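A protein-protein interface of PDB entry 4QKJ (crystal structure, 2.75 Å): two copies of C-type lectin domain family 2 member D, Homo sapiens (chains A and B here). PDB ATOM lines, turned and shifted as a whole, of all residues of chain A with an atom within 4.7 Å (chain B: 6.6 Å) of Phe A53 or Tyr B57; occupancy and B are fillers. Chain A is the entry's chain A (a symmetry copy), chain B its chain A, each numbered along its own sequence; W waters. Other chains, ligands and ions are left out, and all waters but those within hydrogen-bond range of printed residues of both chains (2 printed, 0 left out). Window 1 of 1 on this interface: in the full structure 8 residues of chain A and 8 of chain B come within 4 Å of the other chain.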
ATOM      1  N   ILE A  12      12.201 -31.197   3.827  1.00  0.00           N
ATOM      2  CA  ILE A  12      13.325 -30.329   3.615  1.00  0.00           C
ATOM      3  C   ILE A  12      13.668 -30.377   2.101  1.00  0.00           C
ATOM      4  O   ILE A  12      13.523 -31.432   1.476  1.00  0.00           O
ATOM      5  CB  ILE A  12      14.478 -30.778   4.557  1.00  0.00           C
ATOM      6  CG1 ILE A  12      14.290 -30.198   5.964  1.00  0.00           C
ATOM      7  CG2 ILE A  12      15.859 -30.333   4.057  1.00  0.00           C
ATOM      8  CD1 ILE A  12      13.512 -31.054   6.927  1.00  0.00           C
ATOM      9  N   GLY A  13      14.109 -29.272   1.503  1.00  0.00           N
ATOM     10  CA  GLY A  13      14.377 -29.282   0.077  1.00  0.00           C
ATOM     11  C   GLY A  13      15.814 -29.057  -0.360  1.00  0.00           C
ATOM     12  O   GLY A  13      16.561 -28.207   0.180  1.00  0.00           O
ATOM     13  N   PHE A  14      16.213 -29.804  -1.372  1.00  0.00           N
ATOM     14  CA  PHE A  14      17.577 -29.697  -1.876  1.00  0.00           C
ATOM     15  C   PHE A  14      17.529 -29.986  -3.373  1.00  0.00           C
ATOM     16  O   PHE A  14      16.919 -30.966  -3.771  1.00  0.00           O
ATOM     17  CB  PHE A  14      18.480 -30.709  -1.150  1.00  0.00           C
ATOM     18  CG  PHE A  14      19.887 -30.711  -1.633  1.00  0.00           C
ATOM     19  CD1 PHE A  14      20.724 -29.676  -1.330  1.00  0.00           C
ATOM     20  CD2 PHE A  14      20.374 -31.733  -2.406  1.00  0.00           C
ATOM     21  CE1 PHE A  14      22.046 -29.664  -1.756  1.00  0.00           C
ATOM     22  CE2 PHE A  14      21.701 -31.725  -2.858  1.00  0.00           C
ATOM     23  CZ  PHE A  14      22.539 -30.686  -2.517  1.00  0.00           C
ATOM     24  N   PHE A  19      12.669 -33.957   0.851  1.00  0.00           N
ATOM     25  CA  PHE A  19      12.951 -35.168   1.590  1.00  0.00           C
ATOM     26  C   PHE A  19      12.378 -35.080   2.992  1.00  0.00           C
ATOM     27  O   PHE A  19      12.535 -34.049   3.647  1.00  0.00           O
ATOM     28  CB  PHE A  19      14.433 -35.391   1.749  1.00  0.00           C
ATOM     29  CG  PHE A  19      15.238 -35.331   0.479  1.00  0.00           C
ATOM     30  CD1 PHE A  19      15.526 -34.133  -0.122  1.00  0.00           C
ATOM     31  CD2 PHE A  19      15.811 -36.468  -0.039  1.00  0.00           C
ATOM     32  CE1 PHE A  19      16.327 -34.079  -1.242  1.00  0.00           C
ATOM     33  CE2 PHE A  19      16.603 -36.422  -1.162  1.00  0.00           C
ATOM     34  CZ  PHE A  19      16.866 -35.218  -1.761  1.00  0.00           C
ATOM     35  N   PHE A  21      12.627 -36.715   6.776  1.00  0.00           N
ATOM     36  CA  PHE A  21      13.416 -37.543   7.641  1.00  0.00           C
ATOM     37  C   PHE A  21      12.527 -38.043   8.762  1.00  0.00           C
ATOM     38  O   PHE A  21      11.823 -37.273   9.349  1.00  0.00           O
ATOM     39  CB  PHE A  21      14.581 -36.733   8.138  1.00  0.00           C
ATOM     40  CG  PHE A  21      15.515 -36.263   7.031  1.00  0.00           C
ATOM     41  CD1 PHE A  21      15.258 -35.101   6.342  1.00  0.00           C
ATOM     42  CD2 PHE A  21      16.657 -36.989   6.715  1.00  0.00           C
ATOM     43  CE1 PHE A  21      16.121 -34.659   5.366  1.00  0.00           C
ATOM     44  CE2 PHE A  21      17.513 -36.561   5.725  1.00  0.00           C
ATOM     45  CZ  PHE A  21      17.232 -35.386   5.037  1.00  0.00           C
ATOM     46  N   GLN A  49      25.732 -34.872  -4.325  1.00  0.00           N
ATOM     47  CA  GLN A  49      25.428 -33.838  -3.352  1.00  0.00           C
ATOM     48  C   GLN A  49      24.183 -34.215  -2.585  1.00  0.00           C
ATOM     49  O   GLN A  49      23.941 -33.697  -1.498  1.00  0.00           O
ATOM     50  CB  GLN A  49      25.276 -32.395  -3.951  1.00  0.00           C
ATOM     51  CG  GLN A  49      25.270 -32.175  -5.474  1.00  0.00           C
ATOM     52  CD  GLN A  49      26.653 -32.333  -6.138  1.00  0.00           C
ATOM     53  OE1 GLN A  49      27.680 -31.877  -5.603  1.00  0.00           O
ATOM     54  NE2 GLN A  49      26.677 -32.971  -7.316  1.00  0.00           N
ATOM     55  N   GLU A  50      23.378 -35.106  -3.140  1.00  0.00           N
ATOM     56  CA  GLU A  50      22.151 -35.494  -2.471  1.00  0.00           C
ATOM     57  C   GLU A  50      22.562 -36.406  -1.326  1.00  0.00           C
ATOM     58  O   GLU A  50      21.985 -36.351  -0.247  1.00  0.00           O
ATOM     59  CB  GLU A  50      21.259 -36.207  -3.445  1.00  0.00           C
ATOM     60  CG  GLU A  50      19.834 -36.344  -3.010  1.00  0.00           C
ATOM     61  CD  GLU A  50      19.132 -37.450  -3.762  1.00  0.00           C
ATOM     62  OE1 GLU A  50      19.811 -38.148  -4.569  1.00  0.00           O
ATOM     63  OE2 GLU A  50      17.903 -37.628  -3.552  1.00  0.00           O
ATOM     64  N   LEU A  51      23.595 -37.213  -1.573  1.00  0.00           N
ATOM     65  CA  LEU A  51      24.298 -37.907  -0.508  1.00  0.00           C
ATOM     66  C   LEU A  51      24.723 -36.951   0.557  1.00  0.00           C
ATOM     67  O   LEU A  51      24.177 -37.002   1.639  1.00  0.00           O
ATOM     68  CB  LEU A  51      25.534 -38.630  -0.991  1.00  0.00           C
ATOM     69  CG  LEU A  51      26.129 -39.517   0.077  1.00  0.00           C
ATOM     70  CD1 LEU A  51      25.164 -40.568   0.551  1.00  0.00           C
ATOM     71  CD2 LEU A  51      27.322 -40.208  -0.517  1.00  0.00           C
ATOM     72  N   ASN A  52      25.661 -36.056   0.255  1.00  0.00           N
ATOM     73  CA  ASN A  52      26.204 -35.139   1.282  1.00  0.00           C
ATOM     74  C   ASN A  52      25.077 -34.395   1.993  1.00  0.00           C
ATOM     75  O   ASN A  52      25.100 -34.220   3.202  1.00  0.00           O
ATOM     76  CB  ASN A  52      27.221 -34.168   0.702  1.00  0.00           C
ATOM     77  CG  ASN A  52      27.598 -33.035   1.681  1.00  0.00           C
ATOM     78  OD1 ASN A  52      27.048 -31.910   1.632  1.00  0.00           O
ATOM     79  ND2 ASN A  52      28.552 -33.314   2.548  1.00  0.00           N
ATOM     80  N   PHE A  53      24.043 -34.017   1.292  1.00  0.00           N
ATOM     81  CA  PHE A  53      23.057 -33.252   1.964  1.00  0.00           C
ATOM     82  C   PHE A  53      22.413 -34.132   2.985  1.00  0.00           C
ATOM     83  O   PHE A  53      22.050 -33.662   4.050  1.00  0.00           O
ATOM     84  CB  PHE A  53      22.035 -32.669   0.995  1.00  0.00           C
ATOM     85  CG  PHE A  53      20.655 -32.462   1.583  1.00  0.00           C
ATOM     86  CD1 PHE A  53      20.337 -31.333   2.251  1.00  0.00           C
ATOM     87  CD2 PHE A  53      19.673 -33.394   1.378  1.00  0.00           C
ATOM     88  CE1 PHE A  53      19.060 -31.125   2.741  1.00  0.00           C
ATOM     89  CE2 PHE A  53      18.396 -33.203   1.853  1.00  0.00           C
ATOM     90  CZ  PHE A  53      18.082 -32.052   2.538  1.00  0.00           C
ATOM     91  N   LEU A  54      22.224 -35.396   2.656  1.00  0.00           N
ATOM     92  CA  LEU A  54      21.404 -36.246   3.501  1.00  0.00           C
ATOM     93  C   LEU A  54      22.230 -36.648   4.687  1.00  0.00           C
ATOM     94  O   LEU A  54      21.733 -36.758   5.803  1.00  0.00           O
ATOM     95  CB  LEU A  54      20.991 -37.471   2.738  1.00  0.00           C
ATOM     96  CG  LEU A  54      19.924 -37.268   1.665  1.00  0.00           C
ATOM     97  CD1 LEU A  54      19.772 -38.580   0.929  1.00  0.00           C
ATOM     98  CD2 LEU A  54      18.606 -36.846   2.282  1.00  0.00           C
ATOM     99  N   LEU A  55      23.509 -36.843   4.455  1.00  0.00           N
ATOM    100  CA  LEU A  55      24.413 -37.087   5.542  1.00  0.00           C
ATOM    101  C   LEU A  55      24.379 -35.914   6.485  1.00  0.00           C
ATOM    102  O   LEU A  55      24.253 -36.104   7.675  1.00  0.00           O
ATOM    103  CB  LEU A  55      25.819 -37.351   5.051  1.00  0.00           C
ATOM    104  CG  LEU A  55      25.889 -38.628   4.230  1.00  0.00           C
ATOM    105  CD1 LEU A  55      27.304 -38.821   3.764  1.00  0.00           C
ATOM    106  CD2 LEU A  55      25.470 -39.870   5.005  1.00  0.00           C
ATOM    107  N   ARG A  56      24.454 -34.681   5.984  1.00  0.00           N
ATOM    108  CA  ARG A  56      24.481 -33.546   6.903  1.00  0.00           C
ATOM    109  C   ARG A  56      23.174 -33.374   7.685  1.00  0.00           C
ATOM    110  O   ARG A  56      23.189 -33.239   8.878  1.00  0.00           O
ATOM    111  CB  ARG A  56      24.793 -32.310   6.161  1.00  0.00           C
ATOM    112  CG  ARG A  56      26.256 -31.994   6.091  1.00  0.00           C
ATOM    113  CD  ARG A  56      26.414 -30.603   5.484  1.00  0.00           C
ATOM    114  NE  ARG A  56      26.537 -29.414   6.362  1.00  0.00           N
ATOM    115  CZ  ARG A  56      27.315 -28.360   6.029  1.00  0.00           C
ATOM    116  NH1 ARG A  56      27.404 -27.263   6.772  1.00  0.00           N
ATOM    117  NH2 ARG A  56      27.995 -28.400   4.883  1.00  0.00           N
ATOM    118  N   TYR A  57      22.032 -33.451   7.026  1.00  0.00           N
ATOM    119  CA  TYR A  57      20.782 -33.296   7.713  1.00  0.00           C
ATOM    120  C   TYR A  57      20.374 -34.452   8.582  1.00  0.00           C
ATOM    121  O   TYR A  57      19.638 -34.268   9.575  1.00  0.00           O
ATOM    122  CB  TYR A  57      19.663 -33.059   6.730  1.00  0.00           C
ATOM    123  CG  TYR A  57      18.475 -32.481   7.456  1.00  0.00           C
ATOM    124  CD1 TYR A  57      18.483 -31.193   7.952  1.00  0.00           C
ATOM    125  CD2 TYR A  57      17.353 -33.235   7.686  1.00  0.00           C
ATOM    126  CE1 TYR A  57      17.402 -30.708   8.663  1.00  0.00           C
ATOM    127  CE2 TYR A  57      16.270 -32.720   8.358  1.00  0.00           C
ATOM    128  CZ  TYR A  57      16.315 -31.468   8.857  1.00  0.00           C
ATOM    129  OH  TYR A  57      15.223 -31.019   9.556  1.00  0.00           O
ATOM    130  N   SER B  10      23.727 -25.128  -3.974  1.00  0.00           N
ATOM    131  CA  SER B  10      24.445 -25.151  -2.691  1.00  0.00           C
ATOM    132  C   SER B  10      23.684 -24.489  -1.540  1.00  0.00           C
ATOM    133  O   SER B  10      24.039 -24.641  -0.380  1.00  0.00           O
ATOM    134  CB  SER B  10      25.863 -24.558  -2.828  1.00  0.00           C
ATOM    135  OG  SER B  10      26.716 -25.509  -3.461  1.00  0.00           O
ATOM    136  N   ILE B  12      20.334 -24.173   0.773  1.00  0.00           N
ATOM    137  CA  ILE B  12      19.433 -25.189   1.243  1.00  0.00           C
ATOM    138  C   ILE B  12      18.103 -24.489   1.624  1.00  0.00           C
ATOM    139  O   ILE B  12      18.128 -23.354   2.113  1.00  0.00           O
ATOM    140  CB  ILE B  12      20.122 -25.957   2.407  1.00  0.00           C
ATOM    141  CG1 ILE B  12      21.067 -27.036   1.866  1.00  0.00           C
ATOM    142  CG2 ILE B  12      19.116 -26.649   3.336  1.00  0.00           C
ATOM    143  CD1 ILE B  12      22.493 -26.608   1.644  1.00  0.00           C
ATOM    144  N   GLY B  13      16.952 -25.125   1.411  1.00  0.00           N
ATOM    145  CA  GLY B  13      15.696 -24.463   1.706  1.00  0.00           C
ATOM    146  C   GLY B  13      14.833 -25.067   2.800  1.00  0.00           C
ATOM    147  O   GLY B  13      14.671 -26.303   2.929  1.00  0.00           O
ATOM    148  N   PHE B  19      19.054 -20.877   2.820  1.00  0.00           N
ATOM    149  CA  PHE B  19      20.176 -20.593   3.687  1.00  0.00           C
ATOM    150  C   PHE B  19      21.457 -21.149   3.097  1.00  0.00           C
ATOM    151  O   PHE B  19      21.465 -22.290   2.629  1.00  0.00           O
ATOM    152  CB  PHE B  19      20.013 -21.241   5.038  1.00  0.00           C
ATOM    153  CG  PHE B  19      18.706 -20.971   5.735  1.00  0.00           C
ATOM    154  CD1 PHE B  19      17.551 -21.596   5.343  1.00  0.00           C
ATOM    155  CD2 PHE B  19      18.667 -20.185   6.862  1.00  0.00           C
ATOM    156  CE1 PHE B  19      16.374 -21.401   6.032  1.00  0.00           C
ATOM    157  CE2 PHE B  19      17.493 -19.979   7.548  1.00  0.00           C
ATOM    158  CZ  PHE B  19      16.342 -20.598   7.133  1.00  0.00           C
ATOM    159  N   TYR B  20      22.516 -20.329   3.143  1.00  0.00           N
ATOM    160  CA  TYR B  20      23.864 -20.702   2.807  1.00  0.00           C
ATOM    161  C   TYR B  20      24.610 -21.117   4.065  1.00  0.00           C
ATOM    162  O   TYR B  20      24.576 -20.384   5.061  1.00  0.00           O
ATOM    163  CB  TYR B  20      24.583 -19.475   2.285  1.00  0.00           C
ATOM    164  CG  TYR B  20      26.091 -19.575   1.983  1.00  0.00           C
ATOM    165  CD1 TYR B  20      26.547 -20.129   0.801  1.00  0.00           C
ATOM    166  CD2 TYR B  20      26.999 -19.036   2.798  1.00  0.00           C
ATOM    167  CE1 TYR B  20      27.887 -20.186   0.470  1.00  0.00           C
ATOM    168  CE2 TYR B  20      28.348 -19.100   2.470  1.00  0.00           C
ATOM    169  CZ  TYR B  20      28.782 -19.679   1.295  1.00  0.00           C
ATOM    170  OH  TYR B  20      30.120 -19.753   0.970  1.00  0.00           O
ATOM    171  N   PHE B  21      25.331 -22.237   4.029  1.00  0.00           N
ATOM    172  CA  PHE B  21      26.235 -22.527   5.103  1.00  0.00           C
ATOM    173  C   PHE B  21      27.652 -22.375   4.585  1.00  0.00           C
ATOM    174  O   PHE B  21      27.963 -22.885   3.547  1.00  0.00           O
ATOM    175  CB  PHE B  21      25.944 -23.914   5.605  1.00  0.00           C
ATOM    176  CG  PHE B  21      24.541 -24.075   6.177  1.00  0.00           C
ATOM    177  CD1 PHE B  21      23.478 -24.365   5.354  1.00  0.00           C
ATOM    178  CD2 PHE B  21      24.318 -23.954   7.543  1.00  0.00           C
ATOM    179  CE1 PHE B  21      22.218 -24.544   5.875  1.00  0.00           C
ATOM    180  CE2 PHE B  21      23.054 -24.113   8.066  1.00  0.00           C
ATOM    181  CZ  PHE B  21      21.991 -24.401   7.217  1.00  0.00           C
ATOM    182  N   ASN B  52      16.039 -25.367  14.833  1.00  0.00           N
ATOM    183  CA  ASN B  52      16.306 -26.819  14.733  1.00  0.00           C
ATOM    184  C   ASN B  52      16.847 -27.175  13.351  1.00  0.00           C
ATOM    185  O   ASN B  52      17.765 -27.971  13.219  1.00  0.00           O
ATOM    186  CB  ASN B  52      15.079 -27.651  15.074  1.00  0.00           C
ATOM    187  CG  ASN B  52      15.248 -29.145  14.718  1.00  0.00           C
ATOM    188  OD1 ASN B  52      14.816 -29.620  13.643  1.00  0.00           O
ATOM    189  ND2 ASN B  52      15.846 -29.890  15.628  1.00  0.00           N
ATOM    190  N   PHE B  53      16.361 -26.550  12.313  1.00  0.00           N
ATOM    191  CA  PHE B  53      16.822 -26.968  11.040  1.00  0.00           C
ATOM    192  C   PHE B  53      18.271 -26.620  10.940  1.00  0.00           C
ATOM    193  O   PHE B  53      19.031 -27.352  10.330  1.00  0.00           O
ATOM    194  CB  PHE B  53      16.011 -26.341   9.912  1.00  0.00           C
ATOM    195  CG  PHE B  53      16.776 -26.142   8.619  1.00  0.00           C
ATOM    196  CD1 PHE B  53      16.877 -27.126   7.703  1.00  0.00           C
ATOM    197  CD2 PHE B  53      17.320 -24.920   8.324  1.00  0.00           C
ATOM    198  CE1 PHE B  53      17.531 -26.924   6.501  1.00  0.00           C
ATOM    199  CE2 PHE B  53      17.971 -24.698   7.132  1.00  0.00           C
ATOM    200  CZ  PHE B  53      18.074 -25.709   6.204  1.00  0.00           C
ATOM    201  N   LEU B  54      18.655 -25.485  11.493  1.00  0.00           N
ATOM    202  CA  LEU B  54      19.992 -24.976  11.239  1.00  0.00           C
ATOM    203  C   LEU B  54      20.950 -25.752  12.094  1.00  0.00           C
ATOM    204  O   LEU B  54      22.068 -26.052  11.690  1.00  0.00           O
ATOM    205  CB  LEU B  54      20.057 -23.521  11.603  1.00  0.00           C
ATOM    206  CG  LEU B  54      19.355 -22.556  10.652  1.00  0.00           C
ATOM    207  CD1 LEU B  54      19.414 -21.183  11.281  1.00  0.00           C
ATOM    208  CD2 LEU B  54      20.024 -22.549   9.293  1.00  0.00           C
ATOM    209  N   LEU B  55      20.503 -26.106  13.278  1.00  0.00           N
ATOM    210  CA  LEU B  55      21.281 -26.973  14.116  1.00  0.00           C
ATOM    211  C   LEU B  55      21.512 -28.276  13.399  1.00  0.00           C
ATOM    212  O   LEU B  55      22.629 -28.740  13.343  1.00  0.00           O
ATOM    213  CB  LEU B  55      20.616 -27.198  15.456  1.00  0.00           C
ATOM    214  CG  LEU B  55      20.527 -25.909  16.255  1.00  0.00           C
ATOM    215  CD1 LEU B  55      19.847 -26.201  17.562  1.00  0.00           C
ATOM    216  CD2 LEU B  55      21.885 -25.287  16.554  1.00  0.00           C
ATOM    217  N   ARG B  56      20.481 -28.878  12.805  1.00  0.00           N
ATOM    218  CA  ARG B  56      20.693 -30.171  12.160  1.00  0.00           C
ATOM    219  C   ARG B  56      21.617 -30.090  10.941  1.00  0.00           C
ATOM    220  O   ARG B  56      22.542 -30.846  10.824  1.00  0.00           O
ATOM    221  CB  ARG B  56      19.396 -30.756  11.775  1.00  0.00           C
ATOM    222  CG  ARG B  56      18.788 -31.637  12.823  1.00  0.00           C
ATOM    223  CD  ARG B  56      17.569 -32.328  12.218  1.00  0.00           C
ATOM    224  NE  ARG B  56      17.697 -33.682  11.625  1.00  0.00           N
ATOM    225  CZ  ARG B  56      16.700 -34.591  11.709  1.00  0.00           C
ATOM    226  NH1 ARG B  56      16.768 -35.792  11.145  1.00  0.00           N
ATOM    227  NH2 ARG B  56      15.580 -34.261  12.351  1.00  0.00           N
ATOM    228  N   TYR B  57      21.416 -29.126  10.061  1.00  0.00           N
ATOM    229  CA  TYR B  57      22.253 -29.008   8.902  1.00  0.00           C
ATOM    230  C   TYR B  57      23.644 -28.501   9.158  1.00  0.00           C
ATOM    231  O   TYR B  57      24.584 -28.819   8.398  1.00  0.00           O
ATOM    232  CB  TYR B  57      21.623 -28.090   7.884  1.00  0.00           C
ATOM    233  CG  TYR B  57      22.274 -28.313   6.542  1.00  0.00           C
ATOM    234  CD1 TYR B  57      22.064 -29.468   5.818  1.00  0.00           C
ATOM    235  CD2 TYR B  57      23.133 -27.386   6.011  1.00  0.00           C
ATOM    236  CE1 TYR B  57      22.718 -29.671   4.616  1.00  0.00           C
ATOM    237  CE2 TYR B  57      23.738 -27.585   4.794  1.00  0.00           C
ATOM    238  CZ  TYR B  57      23.540 -28.736   4.119  1.00  0.00           C
ATOM    239  OH  TYR B  57      24.203 -28.902   2.930  1.00  0.00           O
ATOM    240  N   LYS B  58      23.816 -27.653  10.167  1.00  0.00           N
ATOM    241  CA  LYS B  58      25.031 -26.810  10.155  1.00  0.00           C
ATOM    242  C   LYS B  58      26.292 -27.637  10.408  1.00  0.00           C
ATOM    243  O   LYS B  58      27.339 -27.333   9.847  1.00  0.00           O
ATOM    244  CB  LYS B  58      24.922 -25.577  11.056  1.00  0.00           C
ATOM    245  CG  LYS B  58      25.762 -25.609  12.318  1.00  0.00           C
ATOM    246  CD  LYS B  58      24.953 -25.173  13.551  1.00  0.00           C
ATOM    247  CE  LYS B  58      25.838 -24.942  14.773  1.00  0.00           C
ATOM    248  NZ  LYS B  58      26.784 -26.029  15.164  1.00  0.00           N
ATOM    249  N   GLY B  59      26.216 -28.676  11.237  1.00  0.00           N
ATOM    250  CA  GLY B  59      27.437 -29.376  11.597  1.00  0.00           C
ATOM    251  C   GLY B  59      28.151 -28.883  12.866  1.00  0.00           C
ATOM    252  O   GLY B  59      27.637 -28.034  13.647  1.00  0.00           O
HETATM  253  O   HOH W   1      12.995 -35.788  11.476  1.00  0.00           O
HETATM  254  O   HOH W   2      28.702 -25.633   3.609  1.00  0.00           O
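Hydrophobic or aromatic side chains of chain A within 4 Å of the printed part of chain B: Phe A21, Phe A53 and Tyr A57.
Of the 14 printed residues of chain B, 6 touch a printed residue of chain A.
Hydrophobic or aromatic side chains of chain B that line the printed part of chain A: Phe B21, Phe B53 and Tyr B57.
Among the printed residues, 9 pairs touch across the chains.
Phe A21 touches Arg B56, and with the chains exchanged Arg A56 touches Phe B21.
Phe A53 touches Tyr B57, and with the chains exchanged Tyr A57 touches Phe B53.
Arg A56 touches its own counterpart, Arg B56.
Arg A56 touches Tyr B57, and with the chains exchanged Tyr A57 touches Arg B56.
Positions printed for both chains: 12, 13, 19, 21, 52, 53, 54, 55, 56 and 57.
Water W2 bridges the backbone carbonyl oxygen of Phe B21 (2.8 Å) and the guanidinium group of Arg A56 (3.1 Å).
Water W1 bridges O of Phe A21 (2.8 Å) and NH2 of Arg B56 (3.1 Å).
Phe A21 touches Arg B56.
Phe A53 touches Tyr B57.
Arg A56 touches Phe B21 (NH1 to CB, 3.8 Å).
CD1 of Phe B53 touches CE1 of Tyr A57 (3.7 Å).
O of Arg B56 lies close to O of Arg A56 (3.2 Å).
The backbone NH (N) of Gly B13 sits at hydrogen-bond distance from the backbone carbonyl oxygen (O) of Gly A13 (3.3 Å).
The backbone carbonyl oxygen (O) of Tyr B57 is in hydrogen-bond range of the guanidinium group (NE) of Arg A56 (2.9 Å).
The guanidinium group of Arg B56 is in hydrogen-bond range of the backbone carbonyl oxygen of Tyr A57 (2.9 Å).
The backbone carbonyl oxygen (O) of Lys B58 lies within hydrogen-bond range of the guanidinium group (NH1) of Arg A56, at 3.1 Å.
Of the printed residues of chain B, Phe A21 touches Arg B56.
Of chain B, only Tyr B57 (3.7 Å) comes within 4 Å of Phe A53.
Leu A55 touches none of the printed residues of chain B.
Of the printed residues of chain A, Phe B53 touches Tyr A57 (3.7 Å).
Tyr B57 touches just these residues of chain A: Phe A53 (3.7 Å) and Arg A56 (2.9 Å).
Of the printed residues of chain A, Lys B58 touches Arg A56 (3.1 Å).
The nearest residue of chain B that does not touch Phe A53 is Ile B12 (4.4 Å).
The nearest printed residue of chain B that does not touch Gly A13 is Ile B12 (4.3 Å).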
